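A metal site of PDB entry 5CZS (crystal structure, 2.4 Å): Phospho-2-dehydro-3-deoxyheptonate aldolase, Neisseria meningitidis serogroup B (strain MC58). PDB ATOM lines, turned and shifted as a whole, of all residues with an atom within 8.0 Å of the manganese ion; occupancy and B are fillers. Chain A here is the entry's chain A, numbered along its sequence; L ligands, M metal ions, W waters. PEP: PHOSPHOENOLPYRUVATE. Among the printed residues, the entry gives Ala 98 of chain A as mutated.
The manganese ion is bound by water W1. The manganese ion is bound by OE2 of Glu 304 (2.0 Å). The manganese ion is bound by the side-chain carboxylate (OD2) of Asp 324, 2.0 Å away. The manganese ion is bound by a ring nitrogen (NE2) of His 270. The manganese ion is bound by SG of Cys 63 (2.8 Å).
A ring nitrogen (ND1) of His 270 sits close to an oxygen (O2) of the ligand. O1 of the ligand is in salt-bridge range of NH2 of Arg 94 (2.6 Å). An oxygen (O2') of the ligand lies within salt-bridge range of the side-chain amino group (NZ) of Lys 188, 2.7 Å away. NH1 of Arg 167 is in salt-bridge range of O1P of the ligand.
The side-chain carboxylate of Glu 304 lies close to the guanidinium group of Arg 94, 3.8 Å away. The side-chain hydroxyl (OG) of Ser 269 is in hydrogen-bond range of the side-chain carboxylate (OE1) of Glu 304 (2.6 Å). The backbone carbonyl oxygen of Asp 324 is in hydrogen-bond range of the side-chain sulfur of Cys 326 (3.5 Å). The backbone carbonyl oxygen (O) of Asp 324 lies within hydrogen-bond range of the side-chain hydroxyl (OG) of Ser 321 (2.7 Å). A ring nitrogen (ND1) of His 270 is in hydrogen-bond range of the side-chain carboxylate of Asp 267 (2.7 Å). O of Cys 63 sits at hydrogen-bond distance from NH2 of Arg 94 (2.9 Å). The side-chain hydroxyl (OG1) of Thr 323 lies close to the side-chain sulfur (SG) of Cys 63, 2.9 Å away. The side-chain sulfur of Cys 326 sits at hydrogen-bond distance from the backbone NH of Cys 63.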
ATOM      1  N   GLY A  61      30.575   8.398  19.290  1.00  0.00           N
ATOM      2  CA  GLY A  61      29.418   9.195  19.576  1.00  0.00           C
ATOM      3  C   GLY A  61      28.964   8.932  21.002  1.00  0.00           C
ATOM      4  O   GLY A  61      29.655   8.236  21.754  1.00  0.00           O
ATOM      5  N   PRO A  62      27.810   9.466  21.359  1.00  0.00           N
ATOM      6  CA  PRO A  62      27.258   9.331  22.689  1.00  0.00           C
ATOM      7  C   PRO A  62      27.020   7.894  23.148  1.00  0.00           C
ATOM      8  O   PRO A  62      26.687   7.011  22.353  1.00  0.00           O
ATOM      9  CB  PRO A  62      25.914  10.060  22.569  1.00  0.00           C
ATOM     10  CG  PRO A  62      26.166  11.081  21.511  1.00  0.00           C
ATOM     11  CD  PRO A  62      26.938  10.282  20.511  1.00  0.00           C
ATOM     12  N   CYS A  63      27.166   7.691  24.442  1.00  0.00           N
ATOM     13  CA  CYS A  63      26.791   6.427  24.997  1.00  0.00           C
ATOM     14  C   CYS A  63      25.393   6.119  24.571  1.00  0.00           C
ATOM     15  O   CYS A  63      25.079   4.975  24.265  1.00  0.00           O
ATOM     16  CB  CYS A  63      26.858   6.499  26.513  1.00  0.00           C
ATOM     17  SG  CYS A  63      26.225   5.026  27.312  1.00  0.00           S
ATOM     18  N   SER A  64      24.543   7.132  24.575  1.00  0.00           N
ATOM     19  CA  SER A  64      23.151   6.997  24.238  1.00  0.00           C
ATOM     20  C   SER A  64      22.566   8.348  23.828  1.00  0.00           C
ATOM     21  O   SER A  64      22.924   9.405  24.341  1.00  0.00           O
ATOM     22  CB  SER A  64      22.378   6.460  25.415  1.00  0.00           C
ATOM     23  OG  SER A  64      22.103   7.478  26.336  1.00  0.00           O
ATOM     24  N   ARG A  94      27.907   6.706  16.706  1.00  0.00           N
ATOM     25  CA  ARG A  94      27.105   5.927  17.646  1.00  0.00           C
ATOM     26  C   ARG A  94      25.713   6.503  17.746  1.00  0.00           C
ATOM     27  O   ARG A  94      25.568   7.643  18.156  1.00  0.00           O
ATOM     28  CB  ARG A  94      27.725   5.965  19.044  1.00  0.00           C
ATOM     29  CG  ARG A  94      28.865   4.996  19.254  1.00  0.00           C
ATOM     30  CD  ARG A  94      29.317   5.031  20.713  1.00  0.00           C
ATOM     31  NE  ARG A  94      28.261   4.675  21.672  1.00  0.00           N
ATOM     32  CZ  ARG A  94      28.127   3.498  22.264  1.00  0.00           C
ATOM     33  NH1 ARG A  94      28.974   2.519  22.028  1.00  0.00           N
ATOM     34  NH2 ARG A  94      27.128   3.297  23.115  1.00  0.00           N
ATOM     35  N   TYR A  96      22.902   4.904  19.619  1.00  0.00           N
ATOM     36  CA  TYR A  96      22.374   3.899  20.510  1.00  0.00           C
ATOM     37  C   TYR A  96      21.299   4.551  21.338  1.00  0.00           C
ATOM     38  O   TYR A  96      21.529   5.584  21.941  1.00  0.00           O
ATOM     39  CB  TYR A  96      23.469   3.456  21.475  1.00  0.00           C
ATOM     40  CG  TYR A  96      24.523   2.534  20.917  1.00  0.00           C
ATOM     41  CD1 TYR A  96      25.230   2.840  19.772  1.00  0.00           C
ATOM     42  CD2 TYR A  96      24.854   1.359  21.599  1.00  0.00           C
ATOM     43  CE1 TYR A  96      26.209   1.978  19.304  1.00  0.00           C
ATOM     44  CE2 TYR A  96      25.838   0.521  21.146  1.00  0.00           C
ATOM     45  CZ  TYR A  96      26.505   0.831  19.995  1.00  0.00           C
ATOM     46  OH  TYR A  96      27.470  -0.010  19.565  1.00  0.00           O
ATOM     47  N   ALA A  98      19.542   3.182  24.060  1.00  0.00           N
ATOM     48  CA  ALA A  98      19.541   2.824  25.493  1.00  0.00           C
ATOM     49  C   ALA A  98      20.869   2.184  25.977  1.00  0.00           C
ATOM     50  O   ALA A  98      21.638   1.634  25.175  1.00  0.00           O
ATOM     51  CB  ALA A  98      18.360   1.908  25.816  1.00  0.00           C
ATOM     52  N   LYS A  99      21.142   2.262  27.273  1.00  0.00           N
ATOM     53  CA  LYS A  99      22.147   1.392  27.859  1.00  0.00           C
ATOM     54  C   LYS A  99      21.442   0.038  28.049  1.00  0.00           C
ATOM     55  O   LYS A  99      20.252   0.014  28.334  1.00  0.00           O
ATOM     56  CB  LYS A  99      22.664   1.950  29.199  1.00  0.00           C
ATOM     57  N   PRO A 100      22.146  -1.080  27.836  1.00  0.00           N
ATOM     58  CA  PRO A 100      21.569  -2.328  28.370  1.00  0.00           C
ATOM     59  C   PRO A 100      21.756  -2.403  29.911  1.00  0.00           C
ATOM     60  O   PRO A 100      22.735  -3.001  30.396  1.00  0.00           O
ATOM     61  CB  PRO A 100      22.322  -3.426  27.605  1.00  0.00           C
ATOM     62  CG  PRO A 100      23.619  -2.799  27.170  1.00  0.00           C
ATOM     63  CD  PRO A 100      23.437  -1.299  27.157  1.00  0.00           C
ATOM     64  N   ARG A 167      26.402  -8.421  26.967  1.00  0.00           N
ATOM     65  CA  ARG A 167      25.354  -9.160  27.681  1.00  0.00           C
ATOM     66  C   ARG A 167      24.457 -10.037  26.816  1.00  0.00           C
ATOM     67  O   ARG A 167      23.606 -10.720  27.344  1.00  0.00           O
ATOM     68  CB  ARG A 167      24.498  -8.207  28.476  1.00  0.00           C
ATOM     69  CG  ARG A 167      25.324  -7.486  29.533  1.00  0.00           C
ATOM     70  CD  ARG A 167      24.561  -6.343  30.209  1.00  0.00           C
ATOM     71  NE  ARG A 167      25.448  -5.505  31.031  1.00  0.00           N
ATOM     72  CZ  ARG A 167      26.374  -4.653  30.575  1.00  0.00           C
ATOM     73  NH1 ARG A 167      26.610  -4.476  29.274  1.00  0.00           N
ATOM     74  NH2 ARG A 167      27.100  -3.955  31.453  1.00  0.00           N
ATOM     75  N   LYS A 188      30.534  -8.096  20.996  1.00  0.00           N
ATOM     76  CA  LYS A 188      31.410  -7.859  22.141  1.00  0.00           C
ATOM     77  C   LYS A 188      31.750  -9.111  22.950  1.00  0.00           C
ATOM     78  O   LYS A 188      30.985 -10.083  23.000  1.00  0.00           O
ATOM     79  CB  LYS A 188      30.810  -6.835  23.057  1.00  0.00           C
ATOM     80  CG  LYS A 188      30.696  -5.501  22.350  1.00  0.00           C
ATOM     81  CD  LYS A 188      30.445  -4.355  23.305  1.00  0.00           C
ATOM     82  CE  LYS A 188      31.181  -3.096  22.833  1.00  0.00           C
ATOM     83  NZ  LYS A 188      30.840  -1.948  23.685  1.00  0.00           N
ATOM     84  N   ASP A 267      37.119  -1.430  21.879  1.00  0.00           N
ATOM     85  CA  ASP A 267      36.325  -0.403  22.530  1.00  0.00           C
ATOM     86  C   ASP A 267      37.299   0.275  23.486  1.00  0.00           C
ATOM     87  O   ASP A 267      37.949  -0.390  24.309  1.00  0.00           O
ATOM     88  CB  ASP A 267      35.110  -1.045  23.245  1.00  0.00           C
ATOM     89  CG  ASP A 267      34.171  -0.035  23.905  1.00  0.00           C
ATOM     90  OD1 ASP A 267      34.422   1.183  23.784  1.00  0.00           O
ATOM     91  OD2 ASP A 267      33.208  -0.430  24.595  1.00  0.00           O
ATOM     92  N   SER A 269      36.289   2.470  25.606  1.00  0.00           N
ATOM     93  CA  SER A 269      35.478   2.816  26.780  1.00  0.00           C
ATOM     94  C   SER A 269      35.082   1.568  27.539  1.00  0.00           C
ATOM     95  O   SER A 269      35.799   0.552  27.530  1.00  0.00           O
ATOM     96  CB  SER A 269      34.195   3.576  26.360  1.00  0.00           C
ATOM     97  OG  SER A 269      33.588   4.132  27.500  1.00  0.00           O
ATOM     98  N   HIS A 270      33.956   1.664  28.244  1.00  0.00           N
ATOM     99  CA  HIS A 270      33.450   0.580  29.066  1.00  0.00           C
ATOM    100  C   HIS A 270      34.533  -0.092  29.963  1.00  0.00           C
ATOM    101  O   HIS A 270      35.135   0.614  30.793  1.00  0.00           O
ATOM    102  CB  HIS A 270      32.619  -0.322  28.178  1.00  0.00           C
ATOM    103  CG  HIS A 270      31.475   0.404  27.543  1.00  0.00           C
ATOM    104  ND1 HIS A 270      31.485   0.818  26.232  1.00  0.00           N
ATOM    105  CD2 HIS A 270      30.313   0.860  28.070  1.00  0.00           C
ATOM    106  CE1 HIS A 270      30.358   1.454  25.971  1.00  0.00           C
ATOM    107  NE2 HIS A 270      29.632   1.493  27.072  1.00  0.00           N
ATOM    108  N   MET A 302      36.136   1.833  19.145  1.00  0.00           N
ATOM    109  CA  MET A 302      34.885   2.396  19.621  1.00  0.00           C
ATOM    110  C   MET A 302      35.204   3.422  20.697  1.00  0.00           C
ATOM    111  O   MET A 302      36.080   3.193  21.543  1.00  0.00           O
ATOM    112  CB  MET A 302      33.961   1.283  20.117  1.00  0.00           C
ATOM    113  CG  MET A 302      32.592   1.763  20.560  1.00  0.00           C
ATOM    114  SD  MET A 302      31.458   0.405  20.974  1.00  0.00           S
ATOM    115  CE  MET A 302      31.149  -0.292  19.361  1.00  0.00           C
ATOM    116  N   GLU A 304      33.347   6.540  23.279  1.00  0.00           N
ATOM    117  CA  GLU A 304      32.152   7.191  23.771  1.00  0.00           C
ATOM    118  C   GLU A 304      32.432   8.706  23.907  1.00  0.00           C
ATOM    119  O   GLU A 304      33.237   9.111  24.720  1.00  0.00           O
ATOM    120  CB  GLU A 304      31.666   6.552  25.058  1.00  0.00           C
ATOM    121  CG  GLU A 304      30.978   5.200  24.825  1.00  0.00           C
ATOM    122  CD  GLU A 304      30.359   4.629  26.094  1.00  0.00           C
ATOM    123  OE1 GLU A 304      31.085   4.461  27.078  1.00  0.00           O
ATOM    124  OE2 GLU A 304      29.146   4.354  26.102  1.00  0.00           O
ATOM    125  N   SER A 321      26.073  13.517  28.553  1.00  0.00           N
ATOM    126  CA  SER A 321      25.489  12.177  28.696  1.00  0.00           C
ATOM    127  C   SER A 321      24.647  11.972  29.980  1.00  0.00           C
ATOM    128  O   SER A 321      24.985  12.515  31.025  1.00  0.00           O
ATOM    129  CB  SER A 321      26.616  11.150  28.622  1.00  0.00           C
ATOM    130  OG  SER A 321      26.095   9.832  28.619  1.00  0.00           O
ATOM    131  N   THR A 323      23.822   8.611  30.603  1.00  0.00           N
ATOM    132  CA  THR A 323      24.182   7.221  30.821  1.00  0.00           C
ATOM    133  C   THR A 323      25.694   7.274  31.047  1.00  0.00           C
ATOM    134  O   THR A 323      26.128   8.069  31.889  1.00  0.00           O
ATOM    135  CB  THR A 323      23.684   6.372  29.680  1.00  0.00           C
ATOM    136  OG1 THR A 323      24.209   6.859  28.438  1.00  0.00           O
ATOM    137  CG2 THR A 323      22.174   6.435  29.616  1.00  0.00           C
ATOM    138  N   ASP A 324      26.512   6.486  30.327  1.00  0.00           N
ATOM    139  CA  ASP A 324      27.957   6.464  30.637  1.00  0.00           C
ATOM    140  C   ASP A 324      28.656   7.784  30.332  1.00  0.00           C
ATOM    141  O   ASP A 324      28.281   8.516  29.382  1.00  0.00           O
ATOM    142  CB  ASP A 324      28.691   5.356  29.906  1.00  0.00           C
ATOM    143  CG  ASP A 324      28.173   3.953  30.238  1.00  0.00           C
ATOM    144  OD1 ASP A 324      27.813   3.651  31.394  1.00  0.00           O
ATOM    145  OD2 ASP A 324      28.143   3.129  29.294  1.00  0.00           O
ATOM    146  N   ALA A 325      29.671   8.120  31.113  1.00  0.00           N
ATOM    147  CA  ALA A 325      30.399   9.375  30.910  1.00  0.00           C
ATOM    148  C   ALA A 325      31.185   9.299  29.624  1.00  0.00           C
ATOM    149  O   ALA A 325      31.650   8.234  29.255  1.00  0.00           O
ATOM    150  CB  ALA A 325      31.308   9.674  32.080  1.00  0.00           C
ATOM    151  N   CYS A 326      31.312  10.426  28.940  1.00  0.00           N
ATOM    152  CA  CYS A 326      31.958  10.492  27.644  1.00  0.00           C
ATOM    153  C   CYS A 326      33.039  11.571  27.638  1.00  0.00           C
ATOM    154  O   CYS A 326      32.939  12.568  28.379  1.00  0.00           O
ATOM    155  CB  CYS A 326      30.948  10.842  26.544  1.00  0.00           C
ATOM    156  SG  CYS A 326      29.544   9.718  26.308  1.00  0.00           S
HETATM  157  C1  PEP L   1      27.963  -0.064  24.501  1.00  0.00           C
HETATM  158  O1  PEP L   1      27.485   1.097  24.536  1.00  0.00           O
HETATM  159  O2' PEP L   1      28.518  -0.497  23.465  1.00  0.00           O
HETATM  160  C2  PEP L   1      27.890  -0.928  25.691  1.00  0.00           C
HETATM  161  C3  PEP L   1      26.767  -0.999  26.388  1.00  0.00           C
HETATM  162  O2  PEP L   1      29.085  -1.665  26.107  1.00  0.00           O
HETATM  163  P   PEP L   1      29.123  -3.114  26.855  1.00  0.00           P
HETATM  164  O1P PEP L   1      28.684  -2.791  28.278  1.00  0.00           O
HETATM  165  O2P PEP L   1      30.598  -3.425  26.746  1.00  0.00           O
HETATM  166  O3P PEP L   1      28.137  -4.021  26.078  1.00  0.00           O
HETATM  167 MN    MN M   1      28.178   3.075  27.250  1.00  0.00          MN
HETATM  168  O   HOH W   1      26.697   1.912  27.021  1.00  0.00           O
